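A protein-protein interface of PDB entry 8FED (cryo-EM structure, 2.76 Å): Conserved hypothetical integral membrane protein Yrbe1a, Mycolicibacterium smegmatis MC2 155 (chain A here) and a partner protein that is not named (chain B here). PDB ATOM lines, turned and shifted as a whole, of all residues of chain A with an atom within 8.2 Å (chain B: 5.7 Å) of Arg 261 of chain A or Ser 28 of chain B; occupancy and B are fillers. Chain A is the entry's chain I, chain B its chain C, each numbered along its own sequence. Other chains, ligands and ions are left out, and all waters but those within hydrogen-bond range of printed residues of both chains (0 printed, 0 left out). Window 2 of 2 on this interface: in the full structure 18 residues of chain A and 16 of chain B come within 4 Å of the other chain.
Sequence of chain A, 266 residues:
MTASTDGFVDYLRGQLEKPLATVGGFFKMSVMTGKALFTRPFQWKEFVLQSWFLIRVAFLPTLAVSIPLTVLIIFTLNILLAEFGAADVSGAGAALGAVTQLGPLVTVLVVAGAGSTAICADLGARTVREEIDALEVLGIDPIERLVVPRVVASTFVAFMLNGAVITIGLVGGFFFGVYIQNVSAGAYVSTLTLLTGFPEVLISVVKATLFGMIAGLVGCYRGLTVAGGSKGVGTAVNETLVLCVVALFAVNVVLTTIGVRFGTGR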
ATOM      1  N   PRO A 199       3.523   3.667 -20.893  1.00  0.00           N
ATOM      2  CA  PRO A 199       4.815   3.242 -20.324  1.00  0.00           C
ATOM      3  C   PRO A 199       6.007   3.594 -21.197  1.00  0.00           C
ATOM      4  O   PRO A 199       7.065   3.955 -20.670  1.00  0.00           O
ATOM      5  CB  PRO A 199       4.648   1.724 -20.169  1.00  0.00           C
ATOM      6  CG  PRO A 199       3.197   1.521 -20.048  1.00  0.00           C
ATOM      7  CD  PRO A 199       2.575   2.538 -20.947  1.00  0.00           C
ATOM      8  N   GLU A 200       5.862   3.518 -22.523  1.00  0.00           N
ATOM      9  CA  GLU A 200       6.984   3.805 -23.412  1.00  0.00           C
ATOM     10  C   GLU A 200       7.383   5.276 -23.349  1.00  0.00           C
ATOM     11  O   GLU A 200       8.569   5.599 -23.215  1.00  0.00           O
ATOM     12  CB  GLU A 200       6.640   3.400 -24.845  1.00  0.00           C
ATOM     13  CG  GLU A 200       6.895   1.931 -25.163  1.00  0.00           C
ATOM     14  CD  GLU A 200       6.055   0.987 -24.327  1.00  0.00           C
ATOM     15  OE1 GLU A 200       4.903   1.340 -24.004  1.00  0.00           O
ATOM     16  OE2 GLU A 200       6.548  -0.108 -23.986  1.00  0.00           O
ATOM     17  N   VAL A 253      20.862   0.664 -20.891  1.00  0.00           N
ATOM     18  CA  VAL A 253      20.598  -0.773 -20.802  1.00  0.00           C
ATOM     19  C   VAL A 253      19.696  -1.077 -19.609  1.00  0.00           C
ATOM     20  O   VAL A 253      18.701  -1.812 -19.725  1.00  0.00           O
ATOM     21  CB  VAL A 253      21.918  -1.562 -20.726  1.00  0.00           C
ATOM     22  CG1 VAL A 253      21.646  -3.024 -20.416  1.00  0.00           C
ATOM     23  CG2 VAL A 253      22.680  -1.439 -22.029  1.00  0.00           C
ATOM     24  N   VAL A 254      20.023  -0.500 -18.448  1.00  0.00           N
ATOM     25  CA  VAL A 254      19.241  -0.770 -17.239  1.00  0.00           C
ATOM     26  C   VAL A 254      17.801  -0.292 -17.414  1.00  0.00           C
ATOM     27  O   VAL A 254      16.840  -1.017 -17.116  1.00  0.00           O
ATOM     28  CB  VAL A 254      19.905  -0.119 -16.014  1.00  0.00           C
ATOM     29  CG1 VAL A 254      19.054  -0.334 -14.778  1.00  0.00           C
ATOM     30  CG2 VAL A 254      21.297  -0.685 -15.804  1.00  0.00           C
ATOM     31  N   LEU A 255      17.632   0.933 -17.917  1.00  0.00           N
ATOM     32  CA  LEU A 255      16.297   1.491 -18.075  1.00  0.00           C
ATOM     33  C   LEU A 255      15.511   0.781 -19.169  1.00  0.00           C
ATOM     34  O   LEU A 255      14.286   0.689 -19.078  1.00  0.00           O
ATOM     35  CB  LEU A 255      16.383   2.990 -18.351  1.00  0.00           C
ATOM     36  CG  LEU A 255      16.910   3.809 -17.170  1.00  0.00           C
ATOM     37  CD1 LEU A 255      16.930   5.289 -17.495  1.00  0.00           C
ATOM     38  CD2 LEU A 255      16.085   3.545 -15.923  1.00  0.00           C
ATOM     39  N   THR A 256      16.185   0.274 -20.205  1.00  0.00           N
ATOM     40  CA  THR A 256      15.497  -0.513 -21.223  1.00  0.00           C
ATOM     41  C   THR A 256      14.964  -1.813 -20.639  1.00  0.00           C
ATOM     42  O   THR A 256      13.832  -2.214 -20.936  1.00  0.00           O
ATOM     43  CB  THR A 256      16.439  -0.792 -22.393  1.00  0.00           C
ATOM     44  OG1 THR A 256      16.720   0.432 -23.082  1.00  0.00           O
ATOM     45  CG2 THR A 256      15.822  -1.785 -23.366  1.00  0.00           C
ATOM     46  N   THR A 257      15.764  -2.484 -19.805  1.00  0.00           N
ATOM     47  CA  THR A 257      15.275  -3.680 -19.123  1.00  0.00           C
ATOM     48  C   THR A 257      14.058  -3.352 -18.262  1.00  0.00           C
ATOM     49  O   THR A 257      13.031  -4.050 -18.309  1.00  0.00           O
ATOM     50  CB  THR A 257      16.390  -4.292 -18.275  1.00  0.00           C
ATOM     51  OG1 THR A 257      17.510  -4.602 -19.110  1.00  0.00           O
ATOM     52  CG2 THR A 257      15.909  -5.563 -17.601  1.00  0.00           C
ATOM     53  N   ILE A 258      14.153  -2.272 -17.481  1.00  0.00           N
ATOM     54  CA  ILE A 258      13.043  -1.873 -16.619  1.00  0.00           C
ATOM     55  C   ILE A 258      11.798  -1.577 -17.450  1.00  0.00           C
ATOM     56  O   ILE A 258      10.688  -1.999 -17.105  1.00  0.00           O
ATOM     57  CB  ILE A 258      13.449  -0.664 -15.756  1.00  0.00           C
ATOM     58  CG1 ILE A 258      14.543  -1.060 -14.765  1.00  0.00           C
ATOM     59  CG2 ILE A 258      12.248  -0.096 -15.020  1.00  0.00           C
ATOM     60  CD1 ILE A 258      15.041   0.093 -13.926  1.00  0.00           C
ATOM     61  N   GLY A 259      11.966  -0.864 -18.565  1.00  0.00           N
ATOM     62  CA  GLY A 259      10.824  -0.504 -19.387  1.00  0.00           C
ATOM     63  C   GLY A 259      10.161  -1.698 -20.047  1.00  0.00           C
ATOM     64  O   GLY A 259       8.932  -1.787 -20.084  1.00  0.00           O
ATOM     65  N   VAL A 260      10.958  -2.625 -20.589  1.00  0.00           N
ATOM     66  CA  VAL A 260      10.361  -3.802 -21.211  1.00  0.00           C
ATOM     67  C   VAL A 260       9.711  -4.703 -20.174  1.00  0.00           C
ATOM     68  O   VAL A 260       8.849  -5.517 -20.525  1.00  0.00           O
ATOM     69  CB  VAL A 260      11.377  -4.600 -22.052  1.00  0.00           C
ATOM     70  CG1 VAL A 260      11.991  -3.720 -23.128  1.00  0.00           C
ATOM     71  CG2 VAL A 260      12.437  -5.231 -21.175  1.00  0.00           C
ATOM     72  N   ARG A 261      10.102  -4.592 -18.900  1.00  0.00           N
ATOM     73  CA  ARG A 261       9.351  -5.293 -17.862  1.00  0.00           C
ATOM     74  C   ARG A 261       7.915  -4.781 -17.778  1.00  0.00           C
ATOM     75  O   ARG A 261       6.978  -5.571 -17.608  1.00  0.00           O
ATOM     76  CB  ARG A 261      10.065  -5.167 -16.517  1.00  0.00           C
ATOM     77  CG  ARG A 261      10.988  -6.339 -16.229  1.00  0.00           C
ATOM     78  CD  ARG A 261      12.181  -5.939 -15.382  1.00  0.00           C
ATOM     79  NE  ARG A 261      13.085  -7.063 -15.169  1.00  0.00           N
ATOM     80  CZ  ARG A 261      14.310  -6.956 -14.675  1.00  0.00           C
ATOM     81  NH1 ARG A 261      14.821  -5.782 -14.342  1.00  0.00           N
ATOM     82  NH2 ARG A 261      15.045  -8.054 -14.517  1.00  0.00           N
ATOM     83  N   PHE A 262       7.720  -3.470 -17.888  1.00  0.00           N
ATOM     84  CA  PHE A 262       6.379  -2.877 -17.932  1.00  0.00           C
ATOM     85  C   PHE A 262       5.945  -2.632 -19.377  1.00  0.00           C
ATOM     86  O   PHE A 262       5.625  -1.514 -19.777  1.00  0.00           O
ATOM     87  CB  PHE A 262       6.344  -1.582 -17.128  1.00  0.00           C
ATOM     88  CG  PHE A 262       6.903  -1.709 -15.746  1.00  0.00           C
ATOM     89  CD1 PHE A 262       6.156  -2.287 -14.737  1.00  0.00           C
ATOM     90  CD2 PHE A 262       8.168  -1.239 -15.451  1.00  0.00           C
ATOM     91  CE1 PHE A 262       6.665  -2.403 -13.465  1.00  0.00           C
ATOM     92  CE2 PHE A 262       8.685  -1.353 -14.179  1.00  0.00           C
ATOM     93  CZ  PHE A 262       7.932  -1.934 -13.184  1.00  0.00           C
ATOM     94  N   GLY A 263       5.929  -3.704 -20.163  1.00  0.00           N
ATOM     95  CA  GLY A 263       5.660  -3.567 -21.581  1.00  0.00           C
ATOM     96  C   GLY A 263       4.202  -3.265 -21.874  1.00  0.00           C
ATOM     97  O   GLY A 263       3.302  -3.592 -21.102  1.00  0.00           O
ATOM     98  N   THR A 264       3.976  -2.620 -23.021  1.00  0.00           N
ATOM     99  CA  THR A 264       2.612  -2.330 -23.455  1.00  0.00           C
ATOM    100  C   THR A 264       1.887  -3.599 -23.889  1.00  0.00           C
ATOM    101  O   THR A 264       0.721  -3.808 -23.536  1.00  0.00           O
ATOM    102  CB  THR A 264       2.631  -1.305 -24.590  1.00  0.00           C
ATOM    103  OG1 THR A 264       3.089  -0.044 -24.089  1.00  0.00           O
ATOM    104  CG2 THR A 264       1.244  -1.125 -25.187  1.00  0.00           C
ATOM    105  N   ARG A 266       2.363  -6.650 -22.940  1.00  0.00           N
ATOM    106  CA  ARG A 266       2.150  -7.606 -21.860  1.00  0.00           C
ATOM    107  C   ARG A 266       1.371  -6.974 -20.711  1.00  0.00           C
ATOM    108  O   ARG A 266       0.757  -7.672 -19.903  1.00  0.00           O
ATOM    109  CB  ARG A 266       3.487  -8.152 -21.352  1.00  0.00           C
ATOM    110  CG  ARG A 266       4.273  -7.186 -20.487  1.00  0.00           C
ATOM    111  CD  ARG A 266       5.543  -7.832 -19.962  1.00  0.00           C
ATOM    112  NE  ARG A 266       6.498  -8.105 -21.029  1.00  0.00           N
ATOM    113  CZ  ARG A 266       7.668  -8.703 -20.854  1.00  0.00           C
ATOM    114  NH1 ARG A 266       8.060  -9.119 -19.661  1.00  0.00           N
ATOM    115  NH2 ARG A 266       8.463  -8.891 -21.902  1.00  0.00           N
ATOM    116  OXT ARG A 266       1.331  -5.753 -20.563  1.00  0.00           O
ATOM    117  N   ILE B  23      20.314   1.262  -5.957  1.00  0.00           N
ATOM    118  CA  ILE B  23      19.258   1.934  -6.712  1.00  0.00           C
ATOM    119  C   ILE B  23      18.937   1.160  -7.984  1.00  0.00           C
ATOM    120  O   ILE B  23      17.765   0.980  -8.339  1.00  0.00           O
ATOM    121  CB  ILE B  23      19.661   3.390  -7.015  1.00  0.00           C
ATOM    122  CG1 ILE B  23      19.644   4.224  -5.732  1.00  0.00           C
ATOM    123  CG2 ILE B  23      18.739   4.005  -8.055  1.00  0.00           C
ATOM    124  CD1 ILE B  23      20.045   5.665  -5.937  1.00  0.00           C
ATOM    125  N   ILE B  24      19.971   0.689  -8.686  1.00  0.00           N
ATOM    126  CA  ILE B  24      19.753  -0.091  -9.903  1.00  0.00           C
ATOM    127  C   ILE B  24      19.015  -1.385  -9.582  1.00  0.00           C
ATOM    128  O   ILE B  24      18.080  -1.777 -10.292  1.00  0.00           O
ATOM    129  CB  ILE B  24      21.094  -0.355 -10.613  1.00  0.00           C
ATOM    130  CG1 ILE B  24      21.685   0.957 -11.135  1.00  0.00           C
ATOM    131  CG2 ILE B  24      20.921  -1.352 -11.746  1.00  0.00           C
ATOM    132  CD1 ILE B  24      23.009   0.794 -11.843  1.00  0.00           C
ATOM    133  N   GLY B  25      19.414  -2.061  -8.501  1.00  0.00           N
ATOM    134  CA  GLY B  25      18.742  -3.294  -8.122  1.00  0.00           C
ATOM    135  C   GLY B  25      17.287  -3.084  -7.744  1.00  0.00           C
ATOM    136  O   GLY B  25      16.426  -3.902  -8.077  1.00  0.00           O
ATOM    137  N   VAL B  26      16.994  -1.993  -7.032  1.00  0.00           N
ATOM    138  CA  VAL B  26      15.612  -1.691  -6.666  1.00  0.00           C
ATOM    139  C   VAL B  26      14.787  -1.369  -7.905  1.00  0.00           C
ATOM    140  O   VAL B  26      13.662  -1.858  -8.062  1.00  0.00           O
ATOM    141  CB  VAL B  26      15.563  -0.540  -5.645  1.00  0.00           C
ATOM    142  CG1 VAL B  26      14.125  -0.115  -5.391  1.00  0.00           C
ATOM    143  CG2 VAL B  26      16.207  -0.968  -4.353  1.00  0.00           C
ATOM    144  N   GLY B  27      15.331  -0.543  -8.802  1.00  0.00           N
ATOM    145  CA  GLY B  27      14.616  -0.222 -10.024  1.00  0.00           C
ATOM    146  C   GLY B  27      14.351  -1.436 -10.892  1.00  0.00           C
ATOM    147  O   GLY B  27      13.315  -1.513 -11.557  1.00  0.00           O
ATOM    148  N   SER B  28      15.282  -2.393 -10.903  1.00  0.00           N
ATOM    149  CA  SER B  28      15.103  -3.601 -11.700  1.00  0.00           C
ATOM    150  C   SER B  28      13.913  -4.424 -11.220  1.00  0.00           C
ATOM    151  O   SER B  28      13.145  -4.950 -12.033  1.00  0.00           O
ATOM    152  CB  SER B  28      16.381  -4.440 -11.669  1.00  0.00           C
ATOM    153  OG  SER B  28      17.469  -3.732 -12.236  1.00  0.00           O
ATOM    154  N   THR B  29      13.745  -4.548  -9.906  1.00  0.00           N
ATOM    155  CA  THR B  29      12.730  -5.410  -9.300  1.00  0.00           C
ATOM    156  C   THR B  29      11.866  -4.633  -8.316  1.00  0.00           C
ATOM    157  O   THR B  29      11.619  -5.074  -7.191  1.00  0.00           O
ATOM    158  CB  THR B  29      13.370  -6.590  -8.583  1.00  0.00           C
ATOM    159  OG1 THR B  29      14.187  -6.095  -7.517  1.00  0.00           O
ATOM    160  CG2 THR B  29      14.228  -7.405  -9.540  1.00  0.00           C
ATOM    161  N   LEU B  30      11.399  -3.451  -8.720  1.00  0.00           N
ATOM    162  CA  LEU B  30      10.543  -2.672  -7.831  1.00  0.00           C
ATOM    163  C   LEU B  30       9.179  -3.327  -7.647  1.00  0.00           C
ATOM    164  O   LEU B  30       8.553  -3.165  -6.594  1.00  0.00           O
ATOM    165  CB  LEU B  30      10.388  -1.249  -8.370  1.00  0.00           C
ATOM    166  CG  LEU B  30       9.558  -0.267  -7.543  1.00  0.00           C
ATOM    167  CD1 LEU B  30      10.070  -0.205  -6.114  1.00  0.00           C
ATOM    168  CD2 LEU B  30       9.573   1.111  -8.181  1.00  0.00           C
ATOM    169  N   THR B  31       8.707  -4.068  -8.647  1.00  0.00           N
ATOM    170  CA  THR B  31       7.404  -4.715  -8.571  1.00  0.00           C
ATOM    171  C   THR B  31       7.476  -6.112  -7.965  1.00  0.00           C
ATOM    172  O   THR B  31       6.489  -6.584  -7.390  1.00  0.00           O
ATOM    173  CB  THR B  31       6.779  -4.784  -9.967  1.00  0.00           C
ATOM    174  OG1 THR B  31       6.939  -3.518 -10.614  1.00  0.00           O
ATOM    175  CG2 THR B  31       5.292  -5.101  -9.886  1.00  0.00           C
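Printed residues of chain A that touch a printed residue of chain B: Val 254, Ile 258, Arg 261 and Phe 262.
Hydrophobic or aromatic side chains of chain A that line the printed part of chain B: Val 254, Ile 258 and Phe 262.
Of the 9 printed residues of chain B, 4 touch a printed residue of chain A.
The backbone carbonyl oxygen of Ser 28 of chain B is in hydrogen-bond range of the guanidinium group of Arg 261 of chain A (3.0 Å).
Among the printed residues, pairs that only touch across the chains: Val 254 of chain A with Ile 24 of chain B (3.7 Å), Ile 258 of chain A with Gly 27 of chain B (3.3 Å), Ile 258 of chain A with Ser 28 of chain B (3.9 Å) and Phe 262 of chain A with Thr 31 of chain B (3.1 Å).
Printed residues of chain B within 4 Å of Val 254 of chain A: Ile 24 (3.7 Å).
Of the printed residues of chain B, Ile 258 of chain A touches Gly 27 and Ser 28.
Arg 261 of chain A touches just one residue of chain B: Ser 28.
Of chain A, only Ile 258 comes within 4 Å of Gly 27 of chain B.
Ser 28 of chain B touches two residues of chain A.
The nearest residue of chain B that does not touch Arg 261 of chain A is Thr 29 of chain B (4.7 Å).
The nearest residue of chain A that does not touch Ser 28 of chain B is Val 254 of chain A (4.5 Å).
The nearest printed residue of chain A that does not touch Thr 31 of chain B is Arg 261 of chain A (6.9 Å).
OG of Ser 28 of chain B is in hydrogen-bond range of O of Ile 24 of chain B, at 2.8 Å.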
